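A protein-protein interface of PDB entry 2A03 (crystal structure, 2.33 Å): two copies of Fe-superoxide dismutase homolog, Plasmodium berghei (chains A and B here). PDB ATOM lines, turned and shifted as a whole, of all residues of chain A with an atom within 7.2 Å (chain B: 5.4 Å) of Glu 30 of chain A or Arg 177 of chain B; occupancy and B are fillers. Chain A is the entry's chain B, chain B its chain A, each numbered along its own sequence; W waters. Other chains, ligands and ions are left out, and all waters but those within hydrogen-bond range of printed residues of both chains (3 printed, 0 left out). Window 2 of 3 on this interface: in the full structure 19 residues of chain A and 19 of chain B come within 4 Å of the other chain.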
ATOM      1  N   LEU A  20     -14.406   2.361 -22.495  1.00  0.00           N
ATOM      2  CA  LEU A  20     -15.680   1.764 -22.107  1.00  0.00           C
ATOM      3  C   LEU A  20     -16.285   0.832 -23.187  1.00  0.00           C
ATOM      4  O   LEU A  20     -17.011  -0.118 -22.871  1.00  0.00           O
ATOM      5  CB  LEU A  20     -16.678   2.861 -21.743  1.00  0.00           C
ATOM      6  CG  LEU A  20     -16.511   3.583 -20.402  1.00  0.00           C
ATOM      7  CD1 LEU A  20     -17.605   4.635 -20.223  1.00  0.00           C
ATOM      8  CD2 LEU A  20     -16.549   2.615 -19.217  1.00  0.00           C
ATOM      9  N   ASN A  21     -15.981   1.094 -24.453  1.00  0.00           N
ATOM     10  CA  ASN A  21     -16.395   0.208 -25.533  1.00  0.00           C
ATOM     11  C   ASN A  21     -15.360  -0.844 -25.941  1.00  0.00           C
ATOM     12  O   ASN A  21     -15.538  -1.521 -26.959  1.00  0.00           O
ATOM     13  CB  ASN A  21     -16.757   1.026 -26.755  1.00  0.00           C
ATOM     14  CG  ASN A  21     -15.553   1.736 -27.360  1.00  0.00           C
ATOM     15  OD1 ASN A  21     -14.459   1.718 -26.798  1.00  0.00           O
ATOM     16  ND2 ASN A  21     -15.759   2.370 -28.512  1.00  0.00           N
ATOM     17  N   ILE A  27     -18.804  -7.646 -24.114  1.00  0.00           N
ATOM     18  CA  ILE A  27     -19.453  -6.879 -23.048  1.00  0.00           C
ATOM     19  C   ILE A  27     -19.614  -5.482 -23.610  1.00  0.00           C
ATOM     20  O   ILE A  27     -18.632  -4.863 -24.053  1.00  0.00           O
ATOM     21  CB  ILE A  27     -18.649  -6.861 -21.733  1.00  0.00           C
ATOM     22  CG1 ILE A  27     -18.513  -8.275 -21.180  1.00  0.00           C
ATOM     23  CG2 ILE A  27     -19.334  -5.965 -20.682  1.00  0.00           C
ATOM     24  CD1 ILE A  27     -17.570  -8.408 -19.996  1.00  0.00           C
ATOM     25  N   SER A  28     -20.861  -5.010 -23.631  1.00  0.00           N
ATOM     26  CA  SER A  28     -21.211  -3.754 -24.286  1.00  0.00           C
ATOM     27  C   SER A  28     -20.694  -2.554 -23.510  1.00  0.00           C
ATOM     28  O   SER A  28     -20.449  -2.632 -22.313  1.00  0.00           O
ATOM     29  CB  SER A  28     -22.737  -3.622 -24.409  1.00  0.00           C
ATOM     30  OG  SER A  28     -23.312  -3.335 -23.136  1.00  0.00           O
ATOM     31  N   GLU A  29     -20.597  -1.419 -24.182  1.00  0.00           N
ATOM     32  CA  GLU A  29     -20.197  -0.203 -23.504  1.00  0.00           C
ATOM     33  C   GLU A  29     -21.241   0.191 -22.464  1.00  0.00           C
ATOM     34  O   GLU A  29     -20.915   0.762 -21.420  1.00  0.00           O
ATOM     35  CB  GLU A  29     -19.910   0.920 -24.517  1.00  0.00           C
ATOM     36  CG  GLU A  29     -20.899   2.035 -24.548  1.00  0.00           C
ATOM     37  CD  GLU A  29     -20.336   3.322 -23.994  1.00  0.00           C
ATOM     38  OE1 GLU A  29     -19.414   3.914 -24.636  1.00  0.00           O
ATOM     39  OE2 GLU A  29     -20.849   3.754 -22.934  1.00  0.00           O
ATOM     40  N   GLU A  30     -22.497  -0.134 -22.725  1.00  0.00           N
ATOM     41  CA  GLU A  30     -23.536   0.158 -21.752  1.00  0.00           C
ATOM     42  C   GLU A  30     -23.318  -0.603 -20.462  1.00  0.00           C
ATOM     43  O   GLU A  30     -23.406  -0.052 -19.381  1.00  0.00           O
ATOM     44  CB  GLU A  30     -24.895  -0.209 -22.292  1.00  0.00           C
ATOM     45  CG  GLU A  30     -25.976   0.024 -21.267  1.00  0.00           C
ATOM     46  CD  GLU A  30     -27.203   0.600 -21.875  1.00  0.00           C
ATOM     47  OE1 GLU A  30     -27.123   1.030 -23.043  1.00  0.00           O
ATOM     48  OE2 GLU A  30     -28.237   0.645 -21.180  1.00  0.00           O
ATOM     49  N   THR A  31     -23.019  -1.880 -20.574  1.00  0.00           N
ATOM     50  CA  THR A  31     -22.707  -2.654 -19.405  1.00  0.00           C
ATOM     51  C   THR A  31     -21.529  -2.062 -18.626  1.00  0.00           C
ATOM     52  O   THR A  31     -21.654  -1.767 -17.438  1.00  0.00           O
ATOM     53  CB  THR A  31     -22.429  -4.092 -19.786  1.00  0.00           C
ATOM     54  OG1 THR A  31     -23.634  -4.658 -20.314  1.00  0.00           O
ATOM     55  CG2 THR A  31     -21.948  -4.889 -18.568  1.00  0.00           C
ATOM     56  N   LEU A  32     -20.390  -1.883 -19.282  1.00  0.00           N
ATOM     57  CA  LEU A  32     -19.241  -1.270 -18.609  1.00  0.00           C
ATOM     58  C   LEU A  32     -19.577   0.048 -17.957  1.00  0.00           C
ATOM     59  O   LEU A  32     -19.088   0.351 -16.870  1.00  0.00           O
ATOM     60  CB  LEU A  32     -18.104  -1.041 -19.587  1.00  0.00           C
ATOM     61  CG  LEU A  32     -17.006  -2.065 -19.469  1.00  0.00           C
ATOM     62  CD1 LEU A  32     -17.644  -3.381 -19.774  1.00  0.00           C
ATOM     63  CD2 LEU A  32     -15.864  -1.739 -20.439  1.00  0.00           C
ATOM     64  N   SER A  33     -20.404   0.849 -18.619  1.00  0.00           N
ATOM     65  CA  SER A  33     -20.776   2.130 -18.069  1.00  0.00           C
ATOM     66  C   SER A  33     -21.472   1.946 -16.734  1.00  0.00           C
ATOM     67  O   SER A  33     -21.092   2.578 -15.745  1.00  0.00           O
ATOM     68  CB  SER A  33     -21.673   2.896 -19.042  1.00  0.00           C
ATOM     69  OG  SER A  33     -22.218   4.055 -18.409  1.00  0.00           O
ATOM     70  N   PHE A  34     -22.480   1.073 -16.681  1.00  0.00           N
ATOM     71  CA  PHE A  34     -23.149   0.808 -15.418  1.00  0.00           C
ATOM     72  C   PHE A  34     -22.262   0.090 -14.448  1.00  0.00           C
ATOM     73  O   PHE A  34     -22.195   0.428 -13.261  1.00  0.00           O
ATOM     74  CB  PHE A  34     -24.452   0.019 -15.624  1.00  0.00           C
ATOM     75  CG  PHE A  34     -25.628   0.895 -15.689  1.00  0.00           C
ATOM     76  CD1 PHE A  34     -25.995   1.477 -16.894  1.00  0.00           C
ATOM     77  CD2 PHE A  34     -26.306   1.241 -14.535  1.00  0.00           C
ATOM     78  CE1 PHE A  34     -27.057   2.362 -16.955  1.00  0.00           C
ATOM     79  CE2 PHE A  34     -27.385   2.124 -14.589  1.00  0.00           C
ATOM     80  CZ  PHE A  34     -27.757   2.688 -15.796  1.00  0.00           C
ATOM     81  N   HIS A  35     -21.576  -0.923 -14.950  1.00  0.00           N
ATOM     82  CA  HIS A  35     -20.846  -1.807 -14.063  1.00  0.00           C
ATOM     83  C   HIS A  35     -19.702  -1.017 -13.394  1.00  0.00           C
ATOM     84  O   HIS A  35     -19.467  -1.127 -12.193  1.00  0.00           O
ATOM     85  CB  HIS A  35     -20.333  -3.013 -14.851  1.00  0.00           C
ATOM     86  CG  HIS A  35     -20.041  -4.209 -14.004  1.00  0.00           C
ATOM     87  ND1 HIS A  35     -19.813  -5.458 -14.544  1.00  0.00           N
ATOM     88  CD2 HIS A  35     -19.984  -4.357 -12.652  1.00  0.00           C
ATOM     89  CE1 HIS A  35     -19.587  -6.317 -13.559  1.00  0.00           C
ATOM     90  NE2 HIS A  35     -19.707  -5.681 -12.400  1.00  0.00           N
ATOM     91  N   TYR A  36     -18.994  -0.221 -14.182  1.00  0.00           N
ATOM     92  CA  TYR A  36     -17.869   0.574 -13.671  1.00  0.00           C
ATOM     93  C   TYR A  36     -18.329   1.868 -12.985  1.00  0.00           C
ATOM     94  O   TYR A  36     -17.998   2.105 -11.820  1.00  0.00           O
ATOM     95  CB  TYR A  36     -16.912   0.910 -14.814  1.00  0.00           C
ATOM     96  CG  TYR A  36     -15.686   1.682 -14.399  1.00  0.00           C
ATOM     97  CD1 TYR A  36     -14.702   1.090 -13.610  1.00  0.00           C
ATOM     98  CD2 TYR A  36     -15.496   3.009 -14.808  1.00  0.00           C
ATOM     99  CE1 TYR A  36     -13.562   1.807 -13.217  1.00  0.00           C
ATOM    100  CE2 TYR A  36     -14.353   3.717 -14.431  1.00  0.00           C
ATOM    101  CZ  TYR A  36     -13.393   3.101 -13.637  1.00  0.00           C
ATOM    102  OH  TYR A  36     -12.270   3.785 -13.250  1.00  0.00           O
ATOM    103  N   LYS A  38     -21.330   2.982 -12.046  1.00  0.00           N
ATOM    104  CA  LYS A  38     -22.393   2.941 -11.039  1.00  0.00           C
ATOM    105  C   LYS A  38     -22.070   1.936  -9.941  1.00  0.00           C
ATOM    106  O   LYS A  38     -21.930   2.325  -8.776  1.00  0.00           O
ATOM    107  CB  LYS A  38     -23.759   2.632 -11.654  1.00  0.00           C
ATOM    108  CG  LYS A  38     -24.245   3.621 -12.675  1.00  0.00           C
ATOM    109  CD  LYS A  38     -24.614   4.969 -12.071  1.00  0.00           C
ATOM    110  CE  LYS A  38     -25.218   5.877 -13.163  1.00  0.00           C
ATOM    111  NZ  LYS A  38     -25.298   7.320 -12.772  1.00  0.00           N
ATOM    112  N   HIS A  39     -21.947   0.661 -10.294  1.00  0.00           N
ATOM    113  CA  HIS A  39     -21.637  -0.373  -9.307  1.00  0.00           C
ATOM    114  C   HIS A  39     -20.265  -0.192  -8.647  1.00  0.00           C
ATOM    115  O   HIS A  39     -20.172  -0.025  -7.425  1.00  0.00           O
ATOM    116  CB  HIS A  39     -21.755  -1.778  -9.919  1.00  0.00           C
ATOM    117  CG  HIS A  39     -23.167  -2.162 -10.259  1.00  0.00           C
ATOM    118  ND1 HIS A  39     -24.032  -2.707  -9.334  1.00  0.00           N
ATOM    119  CD2 HIS A  39     -23.874  -2.028 -11.407  1.00  0.00           C
ATOM    120  CE1 HIS A  39     -25.208  -2.904  -9.905  1.00  0.00           C
ATOM    121  NE2 HIS A  39     -25.138  -2.501 -11.164  1.00  0.00           N
ATOM    122  N   HIS A 170     -25.825  -8.453 -12.412  1.00  0.00           N
ATOM    123  CA  HIS A 170     -25.528  -7.141 -12.997  1.00  0.00           C
ATOM    124  C   HIS A 170     -24.337  -7.156 -13.954  1.00  0.00           C
ATOM    125  O   HIS A 170     -24.197  -6.249 -14.778  1.00  0.00           O
ATOM    126  CB  HIS A 170     -25.315  -6.087 -11.919  1.00  0.00           C
ATOM    127  CG  HIS A 170     -24.020  -6.220 -11.184  1.00  0.00           C
ATOM    128  ND1 HIS A 170     -23.959  -6.349  -9.815  1.00  0.00           N
ATOM    129  CD2 HIS A 170     -22.738  -6.235 -11.624  1.00  0.00           C
ATOM    130  CE1 HIS A 170     -22.692  -6.450  -9.444  1.00  0.00           C
ATOM    131  NE2 HIS A 170     -21.932  -6.378 -10.522  1.00  0.00           N
ATOM    132  N   TYR A 173     -26.696  -8.852 -17.179  1.00  0.00           N
ATOM    133  CA  TYR A 173     -28.122  -8.814 -17.412  1.00  0.00           C
ATOM    134  C   TYR A 173     -28.471  -7.870 -18.558  1.00  0.00           C
ATOM    135  O   TYR A 173     -29.405  -8.122 -19.299  1.00  0.00           O
ATOM    136  CB  TYR A 173     -28.921  -8.484 -16.133  1.00  0.00           C
ATOM    137  CG  TYR A 173     -30.190  -9.323 -16.071  1.00  0.00           C
ATOM    138  CD1 TYR A 173     -30.128 -10.658 -15.690  1.00  0.00           C
ATOM    139  CD2 TYR A 173     -31.424  -8.812 -16.442  1.00  0.00           C
ATOM    140  CE1 TYR A 173     -31.236 -11.448 -15.664  1.00  0.00           C
ATOM    141  CE2 TYR A 173     -32.551  -9.605 -16.402  1.00  0.00           C
ATOM    142  CZ  TYR A 173     -32.436 -10.942 -16.024  1.00  0.00           C
ATOM    143  OH  TYR A 173     -33.528 -11.773 -15.987  1.00  0.00           O
ATOM    144  N   ILE A 174     -27.703  -6.789 -18.709  1.00  0.00           N
ATOM    145  CA  ILE A 174     -27.986  -5.816 -19.755  1.00  0.00           C
ATOM    146  C   ILE A 174     -27.822  -6.437 -21.145  1.00  0.00           C
ATOM    147  O   ILE A 174     -28.653  -6.245 -22.008  1.00  0.00           O
ATOM    148  CB  ILE A 174     -27.084  -4.559 -19.624  1.00  0.00           C
ATOM    149  CG1 ILE A 174     -27.598  -3.652 -18.495  1.00  0.00           C
ATOM    150  CG2 ILE A 174     -27.021  -3.793 -20.932  1.00  0.00           C
ATOM    151  CD1 ILE A 174     -26.546  -2.690 -17.950  1.00  0.00           C
ATOM    152  N   ASP A 175     -26.749  -7.190 -21.333  1.00  0.00           N
ATOM    153  CA  ASP A 175     -26.416  -7.754 -22.636  1.00  0.00           C
ATOM    154  C   ASP A 175     -27.012  -9.136 -22.885  1.00  0.00           C
ATOM    155  O   ASP A 175     -27.249  -9.483 -24.037  1.00  0.00           O
ATOM    156  CB  ASP A 175     -24.898  -7.881 -22.778  1.00  0.00           C
ATOM    157  CG  ASP A 175     -24.177  -6.552 -22.664  1.00  0.00           C
ATOM    158  OD1 ASP A 175     -24.738  -5.505 -23.051  1.00  0.00           O
ATOM    159  OD2 ASP A 175     -23.024  -6.574 -22.200  1.00  0.00           O
ATOM    160  N   ARG A 177     -29.417 -10.844 -20.467  1.00  0.00           N
ATOM    161  CA  ARG A 177     -30.513 -11.145 -19.566  1.00  0.00           C
ATOM    162  C   ARG A 177     -30.176 -12.371 -18.698  1.00  0.00           C
ATOM    163  O   ARG A 177     -29.156 -12.382 -18.011  1.00  0.00           O
ATOM    164  CB  ARG A 177     -31.804 -11.322 -20.359  1.00  0.00           C
ATOM    165  CG  ARG A 177     -32.247 -10.079 -21.108  1.00  0.00           C
ATOM    166  CD  ARG A 177     -32.763  -9.017 -20.141  1.00  0.00           C
ATOM    167  NE  ARG A 177     -33.346  -7.865 -20.823  1.00  0.00           N
ATOM    168  CZ  ARG A 177     -32.674  -6.765 -21.161  1.00  0.00           C
ATOM    169  NH1 ARG A 177     -31.390  -6.647 -20.885  1.00  0.00           N
ATOM    170  NH2 ARG A 177     -33.282  -5.775 -21.767  1.00  0.00           N
ATOM    171  N   TYR B 172     -35.242  -6.663 -10.865  1.00  0.00           N
ATOM    172  CA  TYR B 172     -35.335  -5.227 -11.166  1.00  0.00           C
ATOM    173  C   TYR B 172     -34.349  -4.664 -12.189  1.00  0.00           C
ATOM    174  O   TYR B 172     -34.503  -3.535 -12.623  1.00  0.00           O
ATOM    175  CB  TYR B 172     -35.247  -4.420  -9.860  1.00  0.00           C
ATOM    176  CG  TYR B 172     -33.944  -4.558  -9.086  1.00  0.00           C
ATOM    177  CD1 TYR B 172     -32.828  -3.756  -9.386  1.00  0.00           C
ATOM    178  CD2 TYR B 172     -33.833  -5.471  -8.033  1.00  0.00           C
ATOM    179  CE1 TYR B 172     -31.646  -3.887  -8.661  1.00  0.00           C
ATOM    180  CE2 TYR B 172     -32.671  -5.604  -7.315  1.00  0.00           C
ATOM    181  CZ  TYR B 172     -31.578  -4.805  -7.614  1.00  0.00           C
ATOM    182  OH  TYR B 172     -30.424  -4.953  -6.875  1.00  0.00           O
ATOM    183  N   TYR B 173     -33.349  -5.432 -12.598  1.00  0.00           N
ATOM    184  CA  TYR B 173     -32.299  -4.873 -13.429  1.00  0.00           C
ATOM    185  C   TYR B 173     -32.797  -4.382 -14.774  1.00  0.00           C
ATOM    186  O   TYR B 173     -32.280  -3.399 -15.302  1.00  0.00           O
ATOM    187  CB  TYR B 173     -31.122  -5.853 -13.625  1.00  0.00           C
ATOM    188  CG  TYR B 173     -29.824  -5.087 -13.600  1.00  0.00           C
ATOM    189  CD1 TYR B 173     -29.233  -4.743 -12.382  1.00  0.00           C
ATOM    190  CD2 TYR B 173     -29.243  -4.620 -14.781  1.00  0.00           C
ATOM    191  CE1 TYR B 173     -28.075  -4.001 -12.345  1.00  0.00           C
ATOM    192  CE2 TYR B 173     -28.085  -3.875 -14.753  1.00  0.00           C
ATOM    193  CZ  TYR B 173     -27.505  -3.567 -13.540  1.00  0.00           C
ATOM    194  OH  TYR B 173     -26.361  -2.834 -13.510  1.00  0.00           O
ATOM    195  N   ILE B 174     -33.781  -5.067 -15.347  1.00  0.00           N
ATOM    196  CA  ILE B 174     -34.310  -4.645 -16.648  1.00  0.00           C
ATOM    197  C   ILE B 174     -34.858  -3.215 -16.583  1.00  0.00           C
ATOM    198  O   ILE B 174     -34.632  -2.411 -17.500  1.00  0.00           O
ATOM    199  CB  ILE B 174     -35.407  -5.596 -17.167  1.00  0.00           C
ATOM    200  CG1 ILE B 174     -34.793  -6.946 -17.549  1.00  0.00           C
ATOM    201  CG2 ILE B 174     -36.094  -4.988 -18.373  1.00  0.00           C
ATOM    202  CD1 ILE B 174     -35.788  -8.023 -17.728  1.00  0.00           C
ATOM    203  N   ASP B 175     -35.564  -2.901 -15.501  1.00  0.00           N
ATOM    204  CA  ASP B 175     -36.277  -1.630 -15.414  1.00  0.00           C
ATOM    205  C   ASP B 175     -35.523  -0.545 -14.673  1.00  0.00           C
ATOM    206  O   ASP B 175     -35.720   0.628 -14.964  1.00  0.00           O
ATOM    207  CB  ASP B 175     -37.638  -1.826 -14.752  1.00  0.00           C
ATOM    208  CG  ASP B 175     -38.427  -2.931 -15.398  1.00  0.00           C
ATOM    209  OD1 ASP B 175     -38.313  -3.034 -16.642  1.00  0.00           O
ATOM    210  OD2 ASP B 175     -39.121  -3.699 -14.669  1.00  0.00           O
ATOM    211  N   TYR B 176     -34.671  -0.927 -13.718  1.00  0.00           N
ATOM    212  CA  TYR B 176     -34.045   0.059 -12.829  1.00  0.00           C
ATOM    213  C   TYR B 176     -32.521  -0.046 -12.728  1.00  0.00           C
ATOM    214  O   TYR B 176     -31.901   0.812 -12.127  1.00  0.00           O
ATOM    215  CB  TYR B 176     -34.651  -0.060 -11.426  1.00  0.00           C
ATOM    216  CG  TYR B 176     -36.129   0.134 -11.415  1.00  0.00           C
ATOM    217  CD1 TYR B 176     -36.676   1.414 -11.581  1.00  0.00           C
ATOM    218  CD2 TYR B 176     -36.996  -0.943 -11.266  1.00  0.00           C
ATOM    219  CE1 TYR B 176     -38.035   1.617 -11.566  1.00  0.00           C
ATOM    220  CE2 TYR B 176     -38.373  -0.752 -11.255  1.00  0.00           C
ATOM    221  CZ  TYR B 176     -38.883   0.533 -11.405  1.00  0.00           C
ATOM    222  OH  TYR B 176     -40.245   0.746 -11.413  1.00  0.00           O
ATOM    223  N   ARG B 177     -31.939  -1.086 -13.337  1.00  0.00           N
ATOM    224  CA  ARG B 177     -30.508  -1.407 -13.194  1.00  0.00           C
ATOM    225  C   ARG B 177     -30.108  -1.481 -11.741  1.00  0.00           C
ATOM    226  O   ARG B 177     -30.708  -2.203 -10.977  1.00  0.00           O
ATOM    227  CB  ARG B 177     -29.601  -0.372 -13.858  1.00  0.00           C
ATOM    228  CG  ARG B 177     -30.055   0.138 -15.165  1.00  0.00           C
ATOM    229  CD  ARG B 177     -30.243  -0.926 -16.099  1.00  0.00           C
ATOM    230  NE  ARG B 177     -29.867  -0.505 -17.430  1.00  0.00           N
ATOM    231  CZ  ARG B 177     -30.160  -1.215 -18.507  1.00  0.00           C
ATOM    232  NH1 ARG B 177     -30.849  -2.361 -18.357  1.00  0.00           N
ATOM    233  NH2 ARG B 177     -29.770  -0.789 -19.713  1.00  0.00           N
ATOM    234  N   ASN B 178     -29.091  -0.707 -11.376  1.00  0.00           N
ATOM    235  CA  ASN B 178     -28.579  -0.685 -10.013  1.00  0.00           C
ATOM    236  C   ASN B 178     -29.468   0.059  -8.991  1.00  0.00           C
ATOM    237  O   ASN B 178     -29.218  -0.004  -7.791  1.00  0.00           O
ATOM    238  CB  ASN B 178     -27.180  -0.074  -9.998  1.00  0.00           C
ATOM    239  CG  ASN B 178     -27.199   1.428 -10.193  1.00  0.00           C
ATOM    240  OD1 ASN B 178     -27.675   1.936 -11.206  1.00  0.00           O
ATOM    241  ND2 ASN B 178     -26.655   2.141  -9.235  1.00  0.00           N
ATOM    242  N   ASP B 179     -30.508   0.737  -9.466  1.00  0.00           N
ATOM    243  CA  ASP B 179     -31.307   1.577  -8.593  1.00  0.00           C
ATOM    244  C   ASP B 179     -32.403   0.757  -7.913  1.00  0.00           C
ATOM    245  O   ASP B 179     -33.601   0.883  -8.218  1.00  0.00           O
ATOM    246  CB  ASP B 179     -31.870   2.738  -9.398  1.00  0.00           C
ATOM    247  CG  ASP B 179     -32.633   3.736  -8.556  1.00  0.00           C
ATOM    248  OD1 ASP B 179     -32.739   3.574  -7.320  1.00  0.00           O
ATOM    249  OD2 ASP B 179     -33.165   4.682  -9.167  1.00  0.00           O
ATOM    250  N   ARG B 180     -31.978  -0.088  -6.981  1.00  0.00           N
ATOM    251  CA  ARG B 180     -32.922  -0.888  -6.197  1.00  0.00           C
ATOM    252  C   ARG B 180     -33.951  -0.030  -5.431  1.00  0.00           C
ATOM    253  O   ARG B 180     -35.097  -0.450  -5.217  1.00  0.00           O
ATOM    254  CB  ARG B 180     -32.172  -1.792  -5.214  1.00  0.00           C
ATOM    255  CG  ARG B 180     -33.009  -2.969  -4.759  1.00  0.00           C
ATOM    256  CD  ARG B 180     -32.370  -3.672  -3.578  1.00  0.00           C
ATOM    257  NE  ARG B 180     -31.205  -4.450  -3.979  1.00  0.00           N
ATOM    258  CZ  ARG B 180     -30.474  -5.188  -3.147  1.00  0.00           C
ATOM    259  NH1 ARG B 180     -30.783  -5.256  -1.850  1.00  0.00           N
ATOM    260  NH2 ARG B 180     -29.425  -5.854  -3.613  1.00  0.00           N
HETATM  261  O   HOH W   1     -33.558  -3.163 -19.914  1.00  0.00           O
HETATM  262  O   HOH W   2     -23.924  -3.239 -14.839  1.00  0.00           O
HETATM  263  O   HOH W   3     -30.903  -3.352 -21.003  1.00  0.00           O
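Phe 34 of chain A touches Arg 177 of chain B (CE2 to CG, 3.4 Å). Phe 34 of chain A touches Asn 178 of chain B (CE2 to OD1, 3.4 Å). Lys 38 of chain A touches Asn 178 of chain B. His 39 of chain A touches Asn 178 of chain B. CB of His 170 of chain A touches CE1 of Tyr 173 of chain B, at 3.5 Å. CE2 of Tyr 173 of chain A touches CG1 of Ile 174 of chain B (3.7 Å). Ile 174 of chain A touches Tyr 173 of chain B (CD1 to CE2, 3.7 Å). Ile 174 of chain A touches Arg 177 of chain B. Arg 177 of chain A touches Ile 174 of chain B.
Water W1 lies within hydrogen-bond range of O of Ile 174 of chain B (2.7 Å), NH2 of Arg 177 of chain A (3.2 Å) and NH1 of Arg 177 of chain B (3.2 Å). Water W2 lies within hydrogen-bond range of the side-chain hydroxyl of Tyr 173 of chain B (2.8 Å), the backbone carbonyl oxygen of His 170 of chain A (3.0 Å) and the backbone NH of His 35 of chain A (3.3 Å). Water W3 bridges NH1 of Arg 177 of chain B (2.8 Å) and NH1 of Arg 177 of chain A (3.3 Å).
A ring nitrogen (NE2) of His 39 of chain A is in hydrogen-bond range of the side-chain hydroxyl of Tyr 173 of chain B (2.7 Å). OE2 of Glu 30 of chain A is in salt-bridge range of NH2 of Arg 177 of chain B, 2.6 Å away.
Tyr 173 of chain A touches Ile 174 of chain B, and with the chains exchanged Ile 174 of chain A touches Tyr 173 of chain B. Ile 174 of chain A touches Arg 177 of chain B, and with the chains exchanged Arg 177 of chain A touches Ile 174 of chain B. Positions printed for both chains: 173, 174, 175 and 177. Of the 11 pairs that touch across the chains among the printed residues, 4 have their exchanged pair printed and touching as well.
Of the 9 printed residues of chain B, 4 touch a printed residue of chain A. Of the 19 printed residues of chain A, 8 touch a printed residue of chain B. Hydrophobic or aromatic side chains of chain A that line the printed part of chain B: Phe 34, His 39, His 170, Tyr 173 and Ile 174.
The side-chain hydroxyl of Ser 28 of chain A sits close to the backbone NH of Glu 30 of chain A (3.3 Å). N of His 39 of chain A sits at hydrogen-bond distance from O of Phe 34 of chain A, 3.0 Å away. The backbone carbonyl oxygen of Tyr 173 of chain A lies within hydrogen-bond range of the guanidinium group of Arg 177 of chain A. The backbone carbonyl oxygen (O) of Ile 174 of chain A is in hydrogen-bond range of the guanidinium group (NH1) of Arg 177 of chain A, at 3.0 Å.
Glu 30 of chain A touches just one residue of chain B: Arg 177. Printed residues of chain B within 4 Å of Lys 38 of chain A: Asn 178. Of the printed residues of chain B, Ile 174 of chain A touches Tyr 173 (3.7 Å) and Arg 177 (3.5 Å). Asp 175 of chain A touches none of the printed residues of chain B. Of the printed residues of chain B, Arg 177 of chain A touches Ile 174 (3.7 Å). Arg 177 of chain B touches three residues of chain A. Asp 179 of chain B touches none of the printed residues of chain A. The nearest residue of chain A that does not touch Arg 177 of chain B is Arg 177 of chain A (5.0 Å).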
